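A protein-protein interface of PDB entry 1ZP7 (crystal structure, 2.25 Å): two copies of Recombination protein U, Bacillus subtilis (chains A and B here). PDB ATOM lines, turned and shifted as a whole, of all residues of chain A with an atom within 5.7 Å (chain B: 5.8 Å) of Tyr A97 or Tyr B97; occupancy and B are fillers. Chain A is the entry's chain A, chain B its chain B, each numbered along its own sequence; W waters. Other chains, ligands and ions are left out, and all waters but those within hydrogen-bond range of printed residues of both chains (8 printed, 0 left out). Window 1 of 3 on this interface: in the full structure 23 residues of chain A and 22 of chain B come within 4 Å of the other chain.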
ATOM      1  N   VAL A  53     -27.314   0.657  -6.741  1.00  0.00           N
ATOM      2  CA  VAL A  53     -25.895   0.866  -6.963  1.00  0.00           C
ATOM      3  C   VAL A  53     -25.115  -0.392  -6.486  1.00  0.00           C
ATOM      4  O   VAL A  53     -24.693  -0.495  -5.326  1.00  0.00           O
ATOM      5  CB  VAL A  53     -25.393   2.161  -6.258  1.00  0.00           C
ATOM      6  CG1 VAL A  53     -23.963   2.401  -6.597  1.00  0.00           C
ATOM      7  CG2 VAL A  53     -26.250   3.392  -6.665  1.00  0.00           C
ATOM      8  N   LYS A  57     -17.011  -6.879  -7.114  1.00  0.00           N
ATOM      9  CA  LYS A  57     -15.686  -6.637  -6.571  1.00  0.00           C
ATOM     10  C   LYS A  57     -14.626  -7.227  -7.515  1.00  0.00           C
ATOM     11  O   LYS A  57     -14.755  -8.390  -7.957  1.00  0.00           O
ATOM     12  CB  LYS A  57     -15.554  -7.253  -5.181  1.00  0.00           C
ATOM     13  CG  LYS A  57     -16.408  -6.599  -4.112  1.00  0.00           C
ATOM     14  CD  LYS A  57     -16.305  -7.353  -2.787  1.00  0.00           C
ATOM     15  CE  LYS A  57     -17.045  -6.615  -1.687  1.00  0.00           C
ATOM     16  NZ  LYS A  57     -16.837  -7.092  -0.247  1.00  0.00           N
ATOM     17  N   TYR A  89     -20.406  -9.675  -5.137  1.00  0.00           N
ATOM     18  CA  TYR A  89     -21.297  -8.574  -5.481  1.00  0.00           C
ATOM     19  C   TYR A  89     -21.882  -7.952  -4.261  1.00  0.00           C
ATOM     20  O   TYR A  89     -22.438  -8.654  -3.435  1.00  0.00           O
ATOM     21  CB  TYR A  89     -22.453  -9.048  -6.359  1.00  0.00           C
ATOM     22  CG  TYR A  89     -22.058  -9.556  -7.720  1.00  0.00           C
ATOM     23  CD1 TYR A  89     -22.092  -8.723  -8.824  1.00  0.00           C
ATOM     24  CD2 TYR A  89     -21.675 -10.893  -7.902  1.00  0.00           C
ATOM     25  CE1 TYR A  89     -21.738  -9.196 -10.072  1.00  0.00           C
ATOM     26  CE2 TYR A  89     -21.310 -11.369  -9.129  1.00  0.00           C
ATOM     27  CZ  TYR A  89     -21.362 -10.531 -10.216  1.00  0.00           C
ATOM     28  OH  TYR A  89     -21.009 -11.036 -11.467  1.00  0.00           O
ATOM     29  N   ASN A  90     -21.767  -6.636  -4.139  1.00  0.00           N
ATOM     30  CA  ASN A  90     -22.540  -5.943  -3.117  1.00  0.00           C
ATOM     31  C   ASN A  90     -22.937  -4.523  -3.518  1.00  0.00           C
ATOM     32  O   ASN A  90     -22.454  -3.969  -4.511  1.00  0.00           O
ATOM     33  CB  ASN A  90     -21.864  -5.993  -1.723  1.00  0.00           C
ATOM     34  CG  ASN A  90     -20.627  -5.090  -1.609  1.00  0.00           C
ATOM     35  OD1 ASN A  90     -20.277  -4.373  -2.530  1.00  0.00           O
ATOM     36  ND2 ASN A  90     -19.968  -5.136  -0.461  1.00  0.00           N
ATOM     37  N   GLY A  91     -23.831  -3.946  -2.739  1.00  0.00           N
ATOM     38  CA  GLY A  91     -24.218  -2.576  -2.978  1.00  0.00           C
ATOM     39  C   GLY A  91     -25.460  -2.198  -2.225  1.00  0.00           C
ATOM     40  O   GLY A  91     -25.770  -2.766  -1.189  1.00  0.00           O
ATOM     41  N   ILE A  92     -26.193  -1.248  -2.767  1.00  0.00           N
ATOM     42  CA  ILE A  92     -27.299  -0.659  -2.013  1.00  0.00           C
ATOM     43  C   ILE A  92     -28.558  -0.589  -2.848  1.00  0.00           C
ATOM     44  O   ILE A  92     -28.504  -0.221  -4.016  1.00  0.00           O
ATOM     45  CB  ILE A  92     -26.914   0.766  -1.473  1.00  0.00           C
ATOM     46  CG1 ILE A  92     -27.975   1.312  -0.504  1.00  0.00           C
ATOM     47  CG2 ILE A  92     -26.570   1.740  -2.609  1.00  0.00           C
ATOM     48  CD1 ILE A  92     -27.697   2.724  -0.047  1.00  0.00           C
ATOM     49  N   TYR A  93     -29.677  -0.970  -2.234  1.00  0.00           N
ATOM     50  CA  TYR A  93     -30.999  -0.754  -2.777  1.00  0.00           C
ATOM     51  C   TYR A  93     -31.881  -0.238  -1.659  1.00  0.00           C
ATOM     52  O   TYR A  93     -32.029  -0.919  -0.641  1.00  0.00           O
ATOM     53  CB  TYR A  93     -31.580  -2.068  -3.337  1.00  0.00           C
ATOM     54  CG  TYR A  93     -32.990  -1.977  -3.894  1.00  0.00           C
ATOM     55  CD1 TYR A  93     -33.294  -1.142  -4.980  1.00  0.00           C
ATOM     56  CD2 TYR A  93     -34.015  -2.731  -3.344  1.00  0.00           C
ATOM     57  CE1 TYR A  93     -34.582  -1.086  -5.512  1.00  0.00           C
ATOM     58  CE2 TYR A  93     -35.317  -2.687  -3.871  1.00  0.00           C
ATOM     59  CZ  TYR A  93     -35.590  -1.860  -4.949  1.00  0.00           C
ATOM     60  OH  TYR A  93     -36.879  -1.801  -5.439  1.00  0.00           O
ATOM     61  N   GLY A  95     -31.717   2.000   0.766  1.00  0.00           N
ATOM     62  CA  GLY A  95     -31.100   1.993   2.081  1.00  0.00           C
ATOM     63  C   GLY A  95     -30.858   0.619   2.696  1.00  0.00           C
ATOM     64  O   GLY A  95     -30.728   0.487   3.920  1.00  0.00           O
ATOM     65  N   ARG A  96     -30.814  -0.421   1.875  1.00  0.00           N
ATOM     66  CA  ARG A  96     -30.405  -1.721   2.395  1.00  0.00           C
ATOM     67  C   ARG A  96     -29.142  -2.196   1.739  1.00  0.00           C
ATOM     68  O   ARG A  96     -28.872  -1.844   0.583  1.00  0.00           O
ATOM     69  CB  ARG A  96     -31.558  -2.731   2.363  1.00  0.00           C
ATOM     70  CG  ARG A  96     -32.695  -2.245   3.315  1.00  0.00           C
ATOM     71  CD  ARG A  96     -33.572  -3.314   3.865  1.00  0.00           C
ATOM     72  NE  ARG A  96     -32.836  -4.341   4.600  1.00  0.00           N
ATOM     73  CZ  ARG A  96     -33.391  -5.468   5.039  1.00  0.00           C
ATOM     74  NH1 ARG A  96     -34.678  -5.699   4.829  1.00  0.00           N
ATOM     75  NH2 ARG A  96     -32.665  -6.370   5.667  1.00  0.00           N
ATOM     76  N   TYR A  97     -28.334  -2.909   2.530  1.00  0.00           N
ATOM     77  CA  TYR A  97     -27.132  -3.577   2.066  1.00  0.00           C
ATOM     78  C   TYR A  97     -27.482  -4.851   1.276  1.00  0.00           C
ATOM     79  O   TYR A  97     -28.185  -5.726   1.775  1.00  0.00           O
ATOM     80  CB  TYR A  97     -26.200  -3.911   3.256  1.00  0.00           C
ATOM     81  CG  TYR A  97     -24.927  -4.657   2.847  1.00  0.00           C
ATOM     82  CD1 TYR A  97     -23.831  -3.965   2.349  1.00  0.00           C
ATOM     83  CD2 TYR A  97     -24.824  -6.053   2.970  1.00  0.00           C
ATOM     84  CE1 TYR A  97     -22.661  -4.615   1.964  1.00  0.00           C
ATOM     85  CE2 TYR A  97     -23.640  -6.723   2.591  1.00  0.00           C
ATOM     86  CZ  TYR A  97     -22.566  -5.994   2.092  1.00  0.00           C
ATOM     87  OH  TYR A  97     -21.398  -6.620   1.682  1.00  0.00           O
ATOM     88  N   ILE A  98     -26.976  -4.942   0.049  1.00  0.00           N
ATOM     89  CA  ILE A  98     -27.256  -6.084  -0.847  1.00  0.00           C
ATOM     90  C   ILE A  98     -25.968  -6.823  -1.109  1.00  0.00           C
ATOM     91  O   ILE A  98     -24.992  -6.204  -1.418  1.00  0.00           O
ATOM     92  CB  ILE A  98     -27.850  -5.633  -2.238  1.00  0.00           C
ATOM     93  CG1 ILE A  98     -28.988  -4.604  -2.051  1.00  0.00           C
ATOM     94  CG2 ILE A  98     -28.309  -6.859  -3.059  1.00  0.00           C
ATOM     95  CD1 ILE A  98     -30.094  -5.083  -1.144  1.00  0.00           C
ATOM     96  N   ASP A  99     -25.977  -8.144  -1.003  1.00  0.00           N
ATOM     97  CA  ASP A  99     -24.744  -8.932  -1.093  1.00  0.00           C
ATOM     98  C   ASP A  99     -25.051 -10.267  -1.760  1.00  0.00           C
ATOM     99  O   ASP A  99     -25.903 -11.002  -1.288  1.00  0.00           O
ATOM    100  CB  ASP A  99     -24.232  -9.188   0.341  1.00  0.00           C
ATOM    101  CG  ASP A  99     -22.826  -9.768   0.382  1.00  0.00           C
ATOM    102  OD1 ASP A  99     -22.618 -10.927  -0.043  1.00  0.00           O
ATOM    103  OD2 ASP A  99     -21.922  -9.048   0.850  1.00  0.00           O
ATOM    104  N   HIS A 123     -18.662 -15.489   5.142  1.00  0.00           N
ATOM    105  CA  HIS A 123     -19.029 -14.087   4.900  1.00  0.00           C
ATOM    106  C   HIS A 123     -20.561 -13.886   4.907  1.00  0.00           C
ATOM    107  O   HIS A 123     -21.105 -13.040   5.644  1.00  0.00           O
ATOM    108  CB  HIS A 123     -18.408 -13.585   3.582  1.00  0.00           C
ATOM    109  CG  HIS A 123     -18.781 -12.173   3.256  1.00  0.00           C
ATOM    110  ND1 HIS A 123     -19.623 -11.842   2.212  1.00  0.00           N
ATOM    111  CD2 HIS A 123     -18.476 -11.011   3.876  1.00  0.00           C
ATOM    112  CE1 HIS A 123     -19.798 -10.535   2.190  1.00  0.00           C
ATOM    113  NE2 HIS A 123     -19.111 -10.006   3.187  1.00  0.00           N
ATOM    114  N   VAL A 127     -23.049 -11.491   7.127  1.00  0.00           N
ATOM    115  CA  VAL A 127     -23.939 -10.459   6.580  1.00  0.00           C
ATOM    116  C   VAL A 127     -25.376 -10.666   7.064  1.00  0.00           C
ATOM    117  O   VAL A 127     -26.035  -9.716   7.479  1.00  0.00           O
ATOM    118  CB  VAL A 127     -23.835 -10.359   5.043  1.00  0.00           C
ATOM    119  CG1 VAL A 127     -24.964  -9.513   4.469  1.00  0.00           C
ATOM    120  CG2 VAL A 127     -22.477  -9.779   4.646  1.00  0.00           C
ATOM    121  N   ASP A 131     -28.460  -8.374   9.438  1.00  0.00           N
ATOM    122  CA  ASP A 131     -29.732  -8.033   8.762  1.00  0.00           C
ATOM    123  C   ASP A 131     -29.527  -7.574   7.297  1.00  0.00           C
ATOM    124  O   ASP A 131     -30.248  -6.718   6.789  1.00  0.00           O
ATOM    125  CB  ASP A 131     -30.486  -6.973   9.592  1.00  0.00           C
ATOM    126  CG  ASP A 131     -31.915  -6.721   9.104  1.00  0.00           C
ATOM    127  OD1 ASP A 131     -32.284  -5.521   9.012  1.00  0.00           O
ATOM    128  OD2 ASP A 131     -32.668  -7.696   8.829  1.00  0.00           O
ATOM    129  N   GLY A 132     -28.537  -8.148   6.627  1.00  0.00           N
ATOM    130  CA  GLY A 132     -28.300  -7.849   5.207  1.00  0.00           C
ATOM    131  C   GLY A 132     -29.189  -8.646   4.278  1.00  0.00           C
ATOM    132  O   GLY A 132     -29.657  -9.731   4.642  1.00  0.00           O
ATOM    133  N   ILE A 133     -29.435  -8.118   3.079  1.00  0.00           N
ATOM    134  CA  ILE A 133     -30.126  -8.892   2.028  1.00  0.00           C
ATOM    135  C   ILE A 133     -29.072  -9.689   1.273  1.00  0.00           C
ATOM    136  O   ILE A 133     -28.288  -9.118   0.516  1.00  0.00           O
ATOM    137  CB  ILE A 133     -31.016  -8.012   1.095  1.00  0.00           C
ATOM    138  CG1 ILE A 133     -32.152  -7.339   1.896  1.00  0.00           C
ATOM    139  CG2 ILE A 133     -31.600  -8.861  -0.022  1.00  0.00           C
ATOM    140  CD1 ILE A 133     -32.938  -6.271   1.148  1.00  0.00           C
ATOM    141  N   CYS A 134     -29.056 -11.003   1.490  1.00  0.00           N
ATOM    142  CA  CYS A 134     -27.942 -11.845   1.075  1.00  0.00           C
ATOM    143  C   CYS A 134     -28.392 -13.179   0.440  1.00  0.00           C
ATOM    144  O   CYS A 134     -29.265 -13.873   0.958  1.00  0.00           O
ATOM    145  CB  CYS A 134     -27.015 -12.112   2.288  1.00  0.00           C
ATOM    146  SG  CYS A 134     -25.425 -12.819   1.866  1.00  0.00           S
ATOM    147  N   VAL B  53     -19.776  -5.667   9.251  1.00  0.00           N
ATOM    148  CA  VAL B  53     -19.045  -6.428   8.242  1.00  0.00           C
ATOM    149  C   VAL B  53     -18.582  -5.469   7.130  1.00  0.00           C
ATOM    150  O   VAL B  53     -19.286  -5.272   6.124  1.00  0.00           O
ATOM    151  CB  VAL B  53     -19.923  -7.585   7.628  1.00  0.00           C
ATOM    152  CG1 VAL B  53     -19.093  -8.520   6.749  1.00  0.00           C
ATOM    153  CG2 VAL B  53     -20.666  -8.362   8.713  1.00  0.00           C
ATOM    154  N   LYS B  57     -12.225  -2.896  -0.652  1.00  0.00           N
ATOM    155  CA  LYS B  57     -12.236  -3.539  -1.955  1.00  0.00           C
ATOM    156  C   LYS B  57     -10.803  -3.750  -2.443  1.00  0.00           C
ATOM    157  O   LYS B  57      -9.930  -2.926  -2.165  1.00  0.00           O
ATOM    158  CB  LYS B  57     -13.029  -2.701  -2.969  1.00  0.00           C
ATOM    159  CG  LYS B  57     -14.531  -2.827  -2.817  1.00  0.00           C
ATOM    160  CD  LYS B  57     -15.259  -1.601  -3.331  1.00  0.00           C
ATOM    161  CE  LYS B  57     -16.720  -1.604  -2.899  1.00  0.00           C
ATOM    162  NZ  LYS B  57     -17.696  -1.753  -4.013  1.00  0.00           N
ATOM    163  N   TYR B  89     -14.083   1.387   0.482  1.00  0.00           N
ATOM    164  CA  TYR B  89     -14.650   0.646   1.608  1.00  0.00           C
ATOM    165  C   TYR B  89     -16.150   0.614   1.537  1.00  0.00           C
ATOM    166  O   TYR B  89     -16.793   1.647   1.314  1.00  0.00           O
ATOM    167  CB  TYR B  89     -14.266   1.277   2.951  1.00  0.00           C
ATOM    168  CG  TYR B  89     -12.789   1.268   3.251  1.00  0.00           C
ATOM    169  CD1 TYR B  89     -12.230   0.276   4.058  1.00  0.00           C
ATOM    170  CD2 TYR B  89     -11.949   2.256   2.722  1.00  0.00           C
ATOM    171  CE1 TYR B  89     -10.869   0.266   4.336  1.00  0.00           C
ATOM    172  CE2 TYR B  89     -10.585   2.250   2.974  1.00  0.00           C
ATOM    173  CZ  TYR B  89     -10.054   1.259   3.788  1.00  0.00           C
ATOM    174  OH  TYR B  89      -8.707   1.255   4.042  1.00  0.00           O
ATOM    175  N   ASN B  90     -16.708  -0.571   1.754  1.00  0.00           N
ATOM    176  CA  ASN B  90     -18.143  -0.690   2.003  1.00  0.00           C
ATOM    177  C   ASN B  90     -18.488  -1.928   2.815  1.00  0.00           C
ATOM    178  O   ASN B  90     -17.631  -2.802   3.057  1.00  0.00           O
ATOM    179  CB  ASN B  90     -18.982  -0.572   0.710  1.00  0.00           C
ATOM    180  CG  ASN B  90     -18.992  -1.860  -0.137  1.00  0.00           C
ATOM    181  OD1 ASN B  90     -18.322  -2.844   0.157  1.00  0.00           O
ATOM    182  ND2 ASN B  90     -19.783  -1.836  -1.204  1.00  0.00           N
ATOM    183  N   GLY B  91     -19.741  -2.008   3.233  1.00  0.00           N
ATOM    184  CA  GLY B  91     -20.160  -3.128   4.025  1.00  0.00           C
ATOM    185  C   GLY B  91     -21.449  -2.797   4.683  1.00  0.00           C
ATOM    186  O   GLY B  91     -22.201  -1.940   4.208  1.00  0.00           O
ATOM    187  N   ILE B  92     -21.699  -3.472   5.790  1.00  0.00           N
ATOM    188  CA  ILE B  92     -22.963  -3.394   6.469  1.00  0.00           C
ATOM    189  C   ILE B  92     -22.752  -3.148   7.950  1.00  0.00           C
ATOM    190  O   ILE B  92     -21.786  -3.633   8.544  1.00  0.00           O
ATOM    191  CB  ILE B  92     -23.838  -4.686   6.198  1.00  0.00           C
ATOM    192  CG1 ILE B  92     -25.208  -4.593   6.868  1.00  0.00           C
ATOM    193  CG2 ILE B  92     -23.093  -5.999   6.560  1.00  0.00           C
ATOM    194  CD1 ILE B  92     -26.177  -5.656   6.387  1.00  0.00           C
ATOM    195  N   TYR B  93     -23.661  -2.361   8.516  1.00  0.00           N
ATOM    196  CA  TYR B  93     -23.770  -2.174   9.945  1.00  0.00           C
ATOM    197  C   TYR B  93     -25.247  -2.013  10.289  1.00  0.00           C
ATOM    198  O   TYR B  93     -25.920  -1.102   9.784  1.00  0.00           O
ATOM    199  CB  TYR B  93     -22.955  -0.959  10.376  1.00  0.00           C
ATOM    200  CG  TYR B  93     -23.156  -0.547  11.812  1.00  0.00           C
ATOM    201  CD1 TYR B  93     -22.671  -1.328  12.858  1.00  0.00           C
ATOM    202  CD2 TYR B  93     -23.820   0.632  12.120  1.00  0.00           C
ATOM    203  CE1 TYR B  93     -22.856  -0.952  14.183  1.00  0.00           C
ATOM    204  CE2 TYR B  93     -24.019   1.019  13.428  1.00  0.00           C
ATOM    205  CZ  TYR B  93     -23.530   0.221  14.460  1.00  0.00           C
ATOM    206  OH  TYR B  93     -23.720   0.610  15.766  1.00  0.00           O
ATOM    207  N   GLY B  95     -28.054  -3.550   9.395  1.00  0.00           N
ATOM    208  CA  GLY B  95     -28.970  -3.546   8.253  1.00  0.00           C
ATOM    209  C   GLY B  95     -28.768  -2.450   7.213  1.00  0.00           C
ATOM    210  O   GLY B  95     -29.442  -2.463   6.170  1.00  0.00           O
ATOM    211  N   ARG B  96     -27.847  -1.515   7.475  1.00  0.00           N
ATOM    212  CA  ARG B  96     -27.571  -0.403   6.553  1.00  0.00           C
ATOM    213  C   ARG B  96     -26.280  -0.559   5.763  1.00  0.00           C
ATOM    214  O   ARG B  96     -25.318  -1.212   6.201  1.00  0.00           O
ATOM    215  CB  ARG B  96     -27.567   0.945   7.273  1.00  0.00           C
ATOM    216  CG  ARG B  96     -28.734   1.173   8.233  1.00  0.00           C
ATOM    217  CD  ARG B  96     -29.880   1.972   7.633  1.00  0.00           C
ATOM    218  NE  ARG B  96     -29.460   3.148   6.849  1.00  0.00           N
ATOM    219  CZ  ARG B  96     -29.513   4.413   7.259  1.00  0.00           C
ATOM    220  NH1 ARG B  96     -29.954   4.707   8.472  1.00  0.00           N
ATOM    221  NH2 ARG B  96     -29.121   5.391   6.446  1.00  0.00           N
ATOM    222  N   TYR B  97     -26.280   0.050   4.586  1.00  0.00           N
ATOM    223  CA  TYR B  97     -25.153   0.018   3.695  1.00  0.00           C
ATOM    224  C   TYR B  97     -24.166   1.142   4.060  1.00  0.00           C
ATOM    225  O   TYR B  97     -24.539   2.305   4.123  1.00  0.00           O
ATOM    226  CB  TYR B  97     -25.653   0.150   2.257  1.00  0.00           C
ATOM    227  CG  TYR B  97     -24.557   0.254   1.241  1.00  0.00           C
ATOM    228  CD1 TYR B  97     -23.987  -0.881   0.675  1.00  0.00           C
ATOM    229  CD2 TYR B  97     -24.081   1.500   0.846  1.00  0.00           C
ATOM    230  CE1 TYR B  97     -22.953  -0.767  -0.259  1.00  0.00           C
ATOM    231  CE2 TYR B  97     -23.089   1.619  -0.050  1.00  0.00           C
ATOM    232  CZ  TYR B  97     -22.522   0.502  -0.622  1.00  0.00           C
ATOM    233  OH  TYR B  97     -21.510   0.684  -1.548  1.00  0.00           O
ATOM    234  N   ILE B  98     -22.908   0.782   4.298  1.00  0.00           N
ATOM    235  CA  ILE B  98     -21.871   1.752   4.686  1.00  0.00           C
ATOM    236  C   ILE B  98     -20.827   1.829   3.575  1.00  0.00           C
ATOM    237  O   ILE B  98     -20.459   0.811   3.001  1.00  0.00           O
ATOM    238  CB  ILE B  98     -21.151   1.347   6.023  1.00  0.00           C
ATOM    239  CG1 ILE B  98     -22.148   0.893   7.110  1.00  0.00           C
ATOM    240  CG2 ILE B  98     -20.189   2.454   6.506  1.00  0.00           C
ATOM    241  CD1 ILE B  98     -23.242   1.904   7.536  1.00  0.00           C
ATOM    242  N   ASP B  99     -20.346   3.032   3.280  1.00  0.00           N
ATOM    243  CA  ASP B  99     -19.467   3.240   2.152  1.00  0.00           C
ATOM    244  C   ASP B  99     -18.594   4.454   2.461  1.00  0.00           C
ATOM    245  O   ASP B  99     -19.080   5.496   2.885  1.00  0.00           O
ATOM    246  CB  ASP B  99     -20.301   3.433   0.881  1.00  0.00           C
ATOM    247  CG  ASP B  99     -19.471   3.517  -0.381  1.00  0.00           C
ATOM    248  OD1 ASP B  99     -18.725   4.509  -0.567  1.00  0.00           O
ATOM    249  OD2 ASP B  99     -19.593   2.610  -1.232  1.00  0.00           O
ATOM    250  N   HIS B 123     -20.062   8.458  -7.350  1.00  0.00           N
ATOM    251  CA  HIS B 123     -20.468   7.234  -6.621  1.00  0.00           C
ATOM    252  C   HIS B 123     -21.057   7.551  -5.229  1.00  0.00           C
ATOM    253  O   HIS B 123     -22.120   7.046  -4.861  1.00  0.00           O
ATOM    254  CB  HIS B 123     -19.308   6.235  -6.521  1.00  0.00           C
ATOM    255  CG  HIS B 123     -19.624   5.034  -5.681  1.00  0.00           C
ATOM    256  ND1 HIS B 123     -19.215   4.912  -4.367  1.00  0.00           N
ATOM    257  CD2 HIS B 123     -20.339   3.915  -5.959  1.00  0.00           C
ATOM    258  CE1 HIS B 123     -19.663   3.767  -3.877  1.00  0.00           C
ATOM    259  NE2 HIS B 123     -20.344   3.146  -4.824  1.00  0.00           N
ATOM    260  N   VAL B 127     -24.788   6.808  -3.668  1.00  0.00           N
ATOM    261  CA  VAL B 127     -25.007   6.051  -2.417  1.00  0.00           C
ATOM    262  C   VAL B 127     -25.884   6.850  -1.447  1.00  0.00           C
ATOM    263  O   VAL B 127     -26.817   6.340  -0.869  1.00  0.00           O
ATOM    264  CB  VAL B 127     -23.652   5.680  -1.734  1.00  0.00           C
ATOM    265  CG1 VAL B 127     -23.881   5.094  -0.326  1.00  0.00           C
ATOM    266  CG2 VAL B 127     -22.866   4.709  -2.603  1.00  0.00           C
ATOM    267  N   ASP B 131     -30.042   6.408  -0.043  1.00  0.00           N
ATOM    268  CA  ASP B 131     -30.212   6.371   1.429  1.00  0.00           C
ATOM    269  C   ASP B 131     -29.138   5.536   2.146  1.00  0.00           C
ATOM    270  O   ASP B 131     -29.412   4.880   3.141  1.00  0.00           O
ATOM    271  CB  ASP B 131     -31.641   5.980   1.849  1.00  0.00           C
ATOM    272  CG  ASP B 131     -32.607   7.187   1.848  1.00  0.00           C
ATOM    273  OD1 ASP B 131     -32.295   8.198   2.519  1.00  0.00           O
ATOM    274  OD2 ASP B 131     -33.676   7.142   1.194  1.00  0.00           O
ATOM    275  N   GLY B 132     -27.913   5.587   1.616  1.00  0.00           N
ATOM    276  CA  GLY B 132     -26.770   4.963   2.251  1.00  0.00           C
ATOM    277  C   GLY B 132     -26.103   5.897   3.250  1.00  0.00           C
ATOM    278  O   GLY B 132     -26.374   7.100   3.276  1.00  0.00           O
ATOM    279  N   ILE B 133     -25.234   5.321   4.071  1.00  0.00           N
ATOM    280  CA  ILE B 133     -24.390   6.065   4.996  1.00  0.00           C
ATOM    281  C   ILE B 133     -23.030   6.152   4.343  1.00  0.00           C
ATOM    282  O   ILE B 133     -22.366   5.142   4.119  1.00  0.00           O
ATOM    283  CB  ILE B 133     -24.298   5.355   6.358  1.00  0.00           C
ATOM    284  CG1 ILE B 133     -25.667   5.363   7.022  1.00  0.00           C
ATOM    285  CG2 ILE B 133     -23.253   6.042   7.263  1.00  0.00           C
ATOM    286  CD1 ILE B 133     -25.859   4.300   8.076  1.00  0.00           C
ATOM    287  N   CYS B 134     -22.622   7.369   4.021  1.00  0.00           N
ATOM    288  CA  CYS B 134     -21.469   7.589   3.195  1.00  0.00           C
ATOM    289  C   CYS B 134     -20.634   8.734   3.784  1.00  0.00           C
ATOM    290  O   CYS B 134     -21.191   9.702   4.297  1.00  0.00           O
ATOM    291  CB  CYS B 134     -21.925   7.895   1.763  1.00  0.00           C
ATOM    292  SG  CYS B 134     -20.604   7.801   0.577  1.00  0.00           S
HETATM  293  O   HOH W   1     -28.368   2.193   4.357  1.00  0.00           O
HETATM  294  O   HOH W   2     -17.694  -5.802   2.051  1.00  0.00           O
HETATM  295  O   HOH W   3     -15.805  -3.956  -0.009  1.00  0.00           O
HETATM  296  O   HOH W   4     -19.573  -6.655   3.673  1.00  0.00           O
HETATM  297  O   HOH W   5     -30.179  -4.543   4.886  1.00  0.00           O
HETATM  298  O   HOH W   6     -20.388  -1.944  -4.469  1.00  0.00           O
HETATM  299  O   HOH W   7     -22.227   0.287  -4.152  1.00  0.00           O
HETATM  300  O   HOH W   8     -18.890  -4.286  -4.778  1.00  0.00           O
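Among the printed residues, merely in contact across the chains: Val A53 with His B123, Asn A90 with Lys B57, Gly A91 with Tyr B97, Ile A92 with Tyr B97, Ile A92 with Val B127, Ile A92 with Asp B131, Ile A92 with Gly B132, Gly A95 with Gly B95, Gly A95 with Asp B131, Arg A96 with Gly B95, Tyr A97 with Gly B91, Tyr A97 with Ile B92, Tyr A97 with Gly B95, Tyr A97 with Tyr B97, His A123 with Val B53, Asp A131 with Ile B92, Asp A131 with Gly B95 and Gly A132 with Ile B92.
Water W5 lies within hydrogen-bond range of O of Gly B95 (2.6 Å), NE of Arg A96 (2.7 Å), O of Asp A131 (2.9 Å) and N of Tyr A97 (3.4 Å).
Water W8 lies within hydrogen-bond range of the side-chain amide oxygen (OD1) of Asn A90 (2.6 Å) and the side-chain amino group (NZ) of Lys B57 (2.9 Å).
Water W4 lies within hydrogen-bond range of the side-chain hydroxyl (OH) of Tyr A97 (2.7 Å), the backbone carbonyl oxygen (O) of Val B53 (2.8 Å) and a ring nitrogen (NE2) of His A123 (3.4 Å).
Water W6 lies within hydrogen-bond range of the side-chain amino group (NZ) of Lys B57 (2.7 Å), the backbone carbonyl oxygen (O) of Asn A90 (2.9 Å) and the side-chain amide nitrogen (ND2) of Asn B90 (3.3 Å).
Water W2 lies within hydrogen-bond range of NZ of Lys A57 (2.8 Å), O of Asn B90 (3.2 Å) and ND2 of Asn A90 (3.5 Å).
Water W1 lies within hydrogen-bond range of NE of Arg B96 (2.9 Å), O of Gly A95 (2.9 Å), N of Tyr B97 (3.0 Å) and O of Asp B131 (3.1 Å).
Tyr A89 touches none of the printed residues of chain B.
Of the printed residues of chain A, Gly B91 touches Tyr A97 (3.2 Å).
Of chain A, only Gly A91, Ile A92 and Tyr A97 come within 4 Å of Tyr B97.
Of the printed residues of chain A, His B123 touches Val A53 (3.98 Å).
Ile B133 touches none of the printed residues of chain A.
The nearest residue of chain B that does not touch Tyr A97 is Arg B96 (4.1 Å).
The nearest printed residue of chain A that does not touch Lys B57 is Lys A57 (4.4 Å).
Asn A90 touches its own counterpart, Asn B90.
Gly B95 touches its own counterpart, Gly A95.
Gly A95 touches Asp B131, and with the chains exchanged Asp A131 touches Gly B95.
Arg A96 touches Gly B95, but with the chains exchanged Gly A95 does not touch Arg B96 (4.1 Å).
Of the 19 pairs that touch across the chains among the printed residues, 15 have their exchanged pair printed and touching as well.
Of the 18 printed residues of chain B, 11 touch a printed residue of chain A.
Among the printed residues, no Asp or Glu carboxylate lies within 4 Å of a Lys or Arg side-chain nitrogen of the other chain.
ND2 of Asn A90 sits at hydrogen-bond distance from OD1 of Asn B90 (2.9 Å).
The backbone carbonyl oxygen (O) of Tyr B97 is in hydrogen-bond range of the backbone NH (N) of Ile B133, at 3.1 Å.
ND2 of Asn A90 is in hydrogen-bond range of OH of Tyr A97, at 3.0 Å.
The backbone NH (N) of Ile B98 lies within hydrogen-bond range of the backbone carbonyl oxygen (O) of Gly B91, at 2.8 Å.
The side-chain hydroxyl (OH) of Tyr A97 lies within hydrogen-bond range of the side-chain carboxylate (OD2) of Asp A99, 2.6 Å away.
O of Ile B92 sits at hydrogen-bond distance from N of Val B53 (2.9 Å).
The backbone NH (N) of Gly A132 is in hydrogen-bond range of the backbone carbonyl oxygen (O) of Val A127, at 3.1 Å.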
